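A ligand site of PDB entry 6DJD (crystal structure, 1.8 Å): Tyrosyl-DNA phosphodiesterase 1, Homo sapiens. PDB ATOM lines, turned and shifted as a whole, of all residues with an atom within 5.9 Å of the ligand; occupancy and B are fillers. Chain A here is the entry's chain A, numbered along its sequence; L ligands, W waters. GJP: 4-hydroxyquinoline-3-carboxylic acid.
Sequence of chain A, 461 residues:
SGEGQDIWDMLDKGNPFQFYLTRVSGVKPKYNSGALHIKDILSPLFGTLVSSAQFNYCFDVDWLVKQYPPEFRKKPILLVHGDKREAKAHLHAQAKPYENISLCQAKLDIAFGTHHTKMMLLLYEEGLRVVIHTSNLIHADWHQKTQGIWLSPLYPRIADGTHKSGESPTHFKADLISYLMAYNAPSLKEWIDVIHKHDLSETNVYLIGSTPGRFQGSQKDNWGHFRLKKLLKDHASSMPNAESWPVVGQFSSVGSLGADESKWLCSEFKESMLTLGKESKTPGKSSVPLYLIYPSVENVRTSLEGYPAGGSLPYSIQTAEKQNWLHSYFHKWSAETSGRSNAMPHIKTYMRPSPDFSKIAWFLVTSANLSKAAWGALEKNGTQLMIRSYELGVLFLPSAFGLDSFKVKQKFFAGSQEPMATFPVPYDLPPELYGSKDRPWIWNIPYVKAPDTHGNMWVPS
The side-chain amide nitrogen of Asn 136 lies within hydrogen-bond range of an oxygen (O2) of the ligand, 2.9 Å away.
O2 of the ligand is in salt-bridge range of NZ of Lys 118 (2.9 Å).
An oxygen (O3) of the ligand is in hydrogen-bond range of a ring nitrogen (NE2) of His 346, at 2.6 Å.
The backbone NH (N) of Asn 136 lies within hydrogen-bond range of the side-chain carboxylate (OD2) of Asp 141 (2.9 Å).
A ring nitrogen (NE2) of His 346 sits close to the side-chain amide nitrogen (ND2) of Asn 136 (3.5 Å).
The backbone carbonyl oxygen (O) of His 116 is in hydrogen-bond range of the side-chain amino group (NZ) of Lys 118, at 2.7 Å.
The side-chain amide oxygen of Asn 136 sits close to the side-chain amide oxygen of Asn 56, 3.3 Å away.
NZ of Lys 348 is in hydrogen-bond range of O of His 346.
OE1 of Glu 391 sits at hydrogen-bond distance from ND1 of His 116 (2.8 Å).
A ring nitrogen (ND1) of His 346 sits at hydrogen-bond distance from the backbone carbonyl oxygen (O) of Thr 134, 2.8 Å away.
Merely in contact with the ligand: Tyr 57, His 116, Gly 311, Ser 312, Pro 314 and Trp 443.
Within 4 Å of the ligand: Tyr 57, His 116, Lys 118, Asn 136, Gly 311, Ser 312, Pro 314, His 346 and Trp 443.
The nearest printed residue that does not touch the ligand is Lys 348 (4.7 Å).
Water W3 lies within hydrogen-bond range of a ring nitrogen (NE2) of His 116 (2.8 Å) and a nitrogen (N) of the ligand (2.9 Å).
Water W4 lies within hydrogen-bond range of the side-chain amino group of Lys 348, the side-chain amide nitrogen of Asn 369, an oxygen (O1) of the ligand, the side-chain hydroxyl of Ser 252 and a ring nitrogen (NE2) of His 346.
Water W1 lies within hydrogen-bond range of OG of Ser 312 (2.8 Å), OD1 of Asp 141 (2.8 Å), O3 of the ligand (3.3 Å) and ND2 of Asn 136 (3.5 Å).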
ATOM      1  N   ASN A  56     -32.327 -13.024 -21.416  1.00  0.00           N
ATOM      2  CA  ASN A  56     -31.493 -12.318 -22.378  1.00  0.00           C
ATOM      3  C   ASN A  56     -30.038 -12.358 -21.942  1.00  0.00           C
ATOM      4  O   ASN A  56     -29.662 -12.986 -20.960  1.00  0.00           O
ATOM      5  CB  ASN A  56     -31.972 -10.886 -22.592  1.00  0.00           C
ATOM      6  CG  ASN A  56     -31.875 -10.479 -24.065  1.00  0.00           C
ATOM      7  OD1 ASN A  56     -30.769 -10.344 -24.577  1.00  0.00           O
ATOM      8  ND2 ASN A  56     -33.019 -10.343 -24.735  1.00  0.00           N
ATOM      9  N   TYR A  57     -29.215 -11.669 -22.725  1.00  0.00           N
ATOM     10  CA  TYR A  57     -27.786 -11.539 -22.464  1.00  0.00           C
ATOM     11  C   TYR A  57     -27.460 -10.147 -21.947  1.00  0.00           C
ATOM     12  O   TYR A  57     -26.895 -10.006 -20.848  1.00  0.00           O
ATOM     13  CB  TYR A  57     -27.018 -11.853 -23.758  1.00  0.00           C
ATOM     14  CG  TYR A  57     -25.549 -11.547 -23.659  1.00  0.00           C
ATOM     15  CD1 TYR A  57     -24.718 -12.311 -22.845  1.00  0.00           C
ATOM     16  CD2 TYR A  57     -24.992 -10.490 -24.367  1.00  0.00           C
ATOM     17  CE1 TYR A  57     -23.368 -12.035 -22.731  1.00  0.00           C
ATOM     18  CE2 TYR A  57     -23.648 -10.201 -24.274  1.00  0.00           C
ATOM     19  CZ  TYR A  57     -22.842 -10.976 -23.461  1.00  0.00           C
ATOM     20  OH  TYR A  57     -21.506 -10.683 -23.367  1.00  0.00           O
ATOM     21  N   HIS A 116     -27.071 -16.780 -23.610  1.00  0.00           N
ATOM     22  CA  HIS A 116     -27.403 -16.081 -24.847  1.00  0.00           C
ATOM     23  C   HIS A 116     -28.881 -16.153 -25.228  1.00  0.00           C
ATOM     24  O   HIS A 116     -29.322 -15.378 -26.077  1.00  0.00           O
ATOM     25  CB  HIS A 116     -26.595 -16.642 -26.019  1.00  0.00           C
ATOM     26  CG  HIS A 116     -25.180 -16.156 -26.106  1.00  0.00           C
ATOM     27  ND1 HIS A 116     -24.165 -16.942 -26.597  1.00  0.00           N
ATOM     28  CD2 HIS A 116     -24.626 -14.960 -25.778  1.00  0.00           C
ATOM     29  CE1 HIS A 116     -23.035 -16.243 -26.576  1.00  0.00           C
ATOM     30  NE2 HIS A 116     -23.283 -15.057 -26.069  1.00  0.00           N
ATOM     31  N   LYS A 118     -32.636 -15.692 -25.888  1.00  0.00           N
ATOM     32  CA  LYS A 118     -33.508 -14.515 -25.917  1.00  0.00           C
ATOM     33  C   LYS A 118     -34.959 -14.967 -26.011  1.00  0.00           C
ATOM     34  O   LYS A 118     -35.401 -15.504 -27.030  1.00  0.00           O
ATOM     35  CB  LYS A 118     -33.078 -13.589 -27.056  1.00  0.00           C
ATOM     36  CG  LYS A 118     -31.645 -13.088 -26.740  1.00  0.00           C
ATOM     37  CD  LYS A 118     -30.983 -12.363 -27.828  1.00  0.00           C
ATOM     38  CE  LYS A 118     -29.576 -11.976 -27.388  1.00  0.00           C
ATOM     39  NZ  LYS A 118     -28.656 -13.122 -27.496  1.00  0.00           N
ATOM     40  N   THR A 134     -34.111 -12.859 -31.194  1.00  0.00           N
ATOM     41  CA  THR A 134     -32.654 -12.762 -31.314  1.00  0.00           C
ATOM     42  C   THR A 134     -32.055 -11.466 -30.780  1.00  0.00           C
ATOM     43  O   THR A 134     -30.836 -11.290 -30.856  1.00  0.00           O
ATOM     44  CB  THR A 134     -32.197 -12.947 -32.785  1.00  0.00           C
ATOM     45  OG1 THR A 134     -32.718 -11.884 -33.616  1.00  0.00           O
ATOM     46  CG2 THR A 134     -32.695 -14.260 -33.326  1.00  0.00           C
ATOM     47  N   ASN A 136     -30.979  -8.422 -28.046  1.00  0.00           N
ATOM     48  CA  ASN A 136     -30.726  -7.938 -26.696  1.00  0.00           C
ATOM     49  C   ASN A 136     -31.745  -6.864 -26.324  1.00  0.00           C
ATOM     50  O   ASN A 136     -32.377  -6.251 -27.176  1.00  0.00           O
ATOM     51  CB  ASN A 136     -29.300  -7.380 -26.579  1.00  0.00           C
ATOM     52  CG  ASN A 136     -28.254  -8.455 -26.719  1.00  0.00           C
ATOM     53  OD1 ASN A 136     -27.971  -9.185 -25.765  1.00  0.00           O
ATOM     54  ND2 ASN A 136     -27.678  -8.592 -27.924  1.00  0.00           N
ATOM     55  N   ASP A 141     -30.332  -2.743 -30.476  1.00  0.00           N
ATOM     56  CA  ASP A 141     -30.636  -4.031 -31.098  1.00  0.00           C
ATOM     57  C   ASP A 141     -31.977  -4.020 -31.811  1.00  0.00           C
ATOM     58  O   ASP A 141     -32.228  -4.909 -32.636  1.00  0.00           O
ATOM     59  CB  ASP A 141     -30.594  -5.156 -30.058  1.00  0.00           C
ATOM     60  CG  ASP A 141     -29.242  -5.874 -30.043  1.00  0.00           C
ATOM     61  OD1 ASP A 141     -28.184  -5.204 -30.167  1.00  0.00           O
ATOM     62  OD2 ASP A 141     -29.232  -7.109 -29.910  1.00  0.00           O
ATOM     63  N   SER A 252     -23.845 -13.951 -36.594  1.00  0.00           N
ATOM     64  CA  SER A 252     -23.226 -12.648 -36.330  1.00  0.00           C
ATOM     65  C   SER A 252     -21.923 -12.754 -35.562  1.00  0.00           C
ATOM     66  O   SER A 252     -21.302 -11.721 -35.297  1.00  0.00           O
ATOM     67  CB  SER A 252     -24.214 -11.747 -35.582  1.00  0.00           C
ATOM     68  OG  SER A 252     -24.512 -12.269 -34.302  1.00  0.00           O
ATOM     69  N   GLY A 311     -19.720  -3.299 -33.569  1.00  0.00           N
ATOM     70  CA  GLY A 311     -19.721  -3.547 -32.146  1.00  0.00           C
ATOM     71  C   GLY A 311     -20.500  -4.780 -31.753  1.00  0.00           C
ATOM     72  O   GLY A 311     -20.220  -5.374 -30.714  1.00  0.00           O
ATOM     73  N   SER A 312     -21.450  -5.204 -32.608  1.00  0.00           N
ATOM     74  CA  SER A 312     -22.305  -6.367 -32.356  1.00  0.00           C
ATOM     75  C   SER A 312     -21.987  -7.536 -33.290  1.00  0.00           C
ATOM     76  O   SER A 312     -22.817  -8.440 -33.457  1.00  0.00           O
ATOM     77  CB  SER A 312     -23.779  -5.970 -32.508  1.00  0.00           C
ATOM     78  OG  SER A 312     -24.154  -4.973 -31.573  1.00  0.00           O
ATOM     79  N   LEU A 313     -20.793  -7.538 -33.874  1.00  0.00           N
ATOM     80  CA  LEU A 313     -20.314  -8.623 -34.729  1.00  0.00           C
ATOM     81  C   LEU A 313     -18.921  -8.955 -34.206  1.00  0.00           C
ATOM     82  O   LEU A 313     -17.919  -8.569 -34.823  1.00  0.00           O
ATOM     83  CB  LEU A 313     -20.280  -8.213 -36.204  1.00  0.00           C
ATOM     84  CG  LEU A 313     -21.613  -7.844 -36.852  1.00  0.00           C
ATOM     85  CD1 LEU A 313     -21.400  -6.958 -38.082  1.00  0.00           C
ATOM     86  CD2 LEU A 313     -22.380  -9.094 -37.241  1.00  0.00           C
ATOM     87  N   PRO A 314     -18.820  -9.646 -33.067  1.00  0.00           N
ATOM     88  CA  PRO A 314     -17.561  -9.671 -32.288  1.00  0.00           C
ATOM     89  C   PRO A 314     -16.604 -10.794 -32.685  1.00  0.00           C
ATOM     90  O   PRO A 314     -16.178 -11.606 -31.848  1.00  0.00           O
ATOM     91  CB  PRO A 314     -18.071  -9.819 -30.852  1.00  0.00           C
ATOM     92  CG  PRO A 314     -19.362 -10.579 -30.981  1.00  0.00           C
ATOM     93  CD  PRO A 314     -19.957 -10.232 -32.333  1.00  0.00           C
ATOM     94  N   HIS A 346     -28.237  -9.385 -36.710  1.00  0.00           N
ATOM     95  CA  HIS A 346     -28.015 -10.002 -35.423  1.00  0.00           C
ATOM     96  C   HIS A 346     -28.897 -11.238 -35.245  1.00  0.00           C
ATOM     97  O   HIS A 346     -28.729 -11.988 -34.276  1.00  0.00           O
ATOM     98  CB  HIS A 346     -28.252  -8.971 -34.311  1.00  0.00           C
ATOM     99  CG  HIS A 346     -27.824  -9.415 -32.939  1.00  0.00           C
ATOM    100  ND1 HIS A 346     -28.709  -9.979 -32.034  1.00  0.00           N
ATOM    101  CD2 HIS A 346     -26.630  -9.342 -32.309  1.00  0.00           C
ATOM    102  CE1 HIS A 346     -28.064 -10.237 -30.907  1.00  0.00           C
ATOM    103  NE2 HIS A 346     -26.801  -9.870 -31.054  1.00  0.00           N
ATOM    104  N   LYS A 348     -29.749 -15.063 -36.247  1.00  0.00           N
ATOM    105  CA  LYS A 348     -28.992 -16.234 -36.703  1.00  0.00           C
ATOM    106  C   LYS A 348     -29.991 -17.211 -37.301  1.00  0.00           C
ATOM    107  O   LYS A 348     -31.036 -17.460 -36.700  1.00  0.00           O
ATOM    108  CB  LYS A 348     -28.194 -16.927 -35.567  1.00  0.00           C
ATOM    109  CG  LYS A 348     -27.151 -16.025 -34.891  1.00  0.00           C
ATOM    110  CD  LYS A 348     -27.765 -15.215 -33.752  1.00  0.00           C
ATOM    111  CE  LYS A 348     -26.667 -14.445 -33.008  1.00  0.00           C
ATOM    112  NZ  LYS A 348     -27.142 -13.127 -32.535  1.00  0.00           N
ATOM    113  N   SER A 367     -30.677 -18.136 -31.314  1.00  0.00           N
ATOM    114  CA  SER A 367     -29.628 -17.283 -30.779  1.00  0.00           C
ATOM    115  C   SER A 367     -28.227 -17.810 -31.076  1.00  0.00           C
ATOM    116  O   SER A 367     -27.250 -17.082 -30.909  1.00  0.00           O
ATOM    117  CB  SER A 367     -29.805 -17.146 -29.249  1.00  0.00           C
ATOM    118  OG  SER A 367     -29.685 -18.429 -28.633  1.00  0.00           O
ATOM    119  N   ASN A 369     -24.824 -18.699 -32.509  1.00  0.00           N
ATOM    120  CA  ASN A 369     -23.826 -18.345 -33.508  1.00  0.00           C
ATOM    121  C   ASN A 369     -23.050 -19.578 -33.956  1.00  0.00           C
ATOM    122  O   ASN A 369     -23.315 -20.701 -33.519  1.00  0.00           O
ATOM    123  CB  ASN A 369     -22.889 -17.256 -32.959  1.00  0.00           C
ATOM    124  CG  ASN A 369     -23.478 -15.881 -33.099  1.00  0.00           C
ATOM    125  OD1 ASN A 369     -24.001 -15.525 -34.158  1.00  0.00           O
ATOM    126  ND2 ASN A 369     -23.408 -15.085 -32.034  1.00  0.00           N
ATOM    127  N   GLU A 391     -28.594 -21.398 -25.209  1.00  0.00           N
ATOM    128  CA  GLU A 391     -29.070 -20.908 -26.501  1.00  0.00           C
ATOM    129  C   GLU A 391     -30.493 -21.408 -26.716  1.00  0.00           C
ATOM    130  O   GLU A 391     -30.891 -22.423 -26.140  1.00  0.00           O
ATOM    131  CB  GLU A 391     -28.213 -21.402 -27.698  1.00  0.00           C
ATOM    132  CG  GLU A 391     -26.723 -21.204 -27.543  1.00  0.00           C
ATOM    133  CD  GLU A 391     -26.268 -19.775 -27.830  1.00  0.00           C
ATOM    134  OE1 GLU A 391     -25.077 -19.457 -27.561  1.00  0.00           O
ATOM    135  OE2 GLU A 391     -27.088 -18.960 -28.301  1.00  0.00           O
ATOM    136  N   TRP A 443     -13.739  -7.215 -35.429  1.00  0.00           N
ATOM    137  CA  TRP A 443     -14.167  -6.036 -34.699  1.00  0.00           C
ATOM    138  C   TRP A 443     -13.033  -5.311 -33.986  1.00  0.00           C
ATOM    139  O   TRP A 443     -13.206  -4.135 -33.647  1.00  0.00           O
ATOM    140  CB  TRP A 443     -15.286  -6.365 -33.684  1.00  0.00           C
ATOM    141  CG  TRP A 443     -14.900  -7.088 -32.405  1.00  0.00           C
ATOM    142  CD1 TRP A 443     -13.844  -7.948 -32.227  1.00  0.00           C
ATOM    143  CD2 TRP A 443     -15.593  -7.027 -31.148  1.00  0.00           C
ATOM    144  NE1 TRP A 443     -13.846  -8.425 -30.923  1.00  0.00           N
ATOM    145  CE2 TRP A 443     -14.901  -7.869 -30.252  1.00  0.00           C
ATOM    146  CE3 TRP A 443     -16.723  -6.344 -30.705  1.00  0.00           C
ATOM    147  CZ2 TRP A 443     -15.311  -8.040 -28.923  1.00  0.00           C
ATOM    148  CZ3 TRP A 443     -17.129  -6.505 -29.375  1.00  0.00           C
ATOM    149  CH2 TRP A 443     -16.426  -7.350 -28.509  1.00  0.00           C
HETATM  150  C4  GJP L   1     -21.678 -10.227 -27.613  1.00  0.00           C
HETATM  151  C5  GJP L   1     -20.392  -9.671 -27.451  1.00  0.00           C
HETATM  152  C6  GJP L   1     -20.047  -8.492 -28.103  1.00  0.00           C
HETATM  153  C7  GJP L   1     -20.970  -7.854 -28.916  1.00  0.00           C
HETATM  154  C8  GJP L   1     -22.239  -8.394 -29.086  1.00  0.00           C
HETATM  155  C9  GJP L   1     -22.592  -9.592 -28.425  1.00  0.00           C
HETATM  156  C10 GJP L   1     -23.869 -10.152 -28.577  1.00  0.00           C
HETATM  157  C3  GJP L   1     -23.187 -11.924 -27.106  1.00  0.00           C
HETATM  158  N   GJP L   1     -21.999 -11.371 -26.979  1.00  0.00           N
HETATM  159  C1  GJP L   1     -25.549 -12.010 -28.043  1.00  0.00           C
HETATM  160  C2  GJP L   1     -24.178 -11.346 -27.904  1.00  0.00           C
HETATM  161  O1  GJP L   1     -25.673 -13.264 -27.996  1.00  0.00           O
HETATM  162  O2  GJP L   1     -26.561 -11.285 -28.235  1.00  0.00           O
HETATM  163  O3  GJP L   1     -24.820  -9.503 -29.390  1.00  0.00           O
HETATM  164  O   HOH W   1     -25.695  -6.364 -29.734  1.00  0.00           O
HETATM  165  O   HOH W   2     -20.351  -8.116 -24.505  1.00  0.00           O
HETATM  166  O   HOH W   3     -20.820 -13.735 -25.872  1.00  0.00           O
HETATM  167  O   HOH W   4     -24.797 -12.714 -30.965  1.00  0.00           O
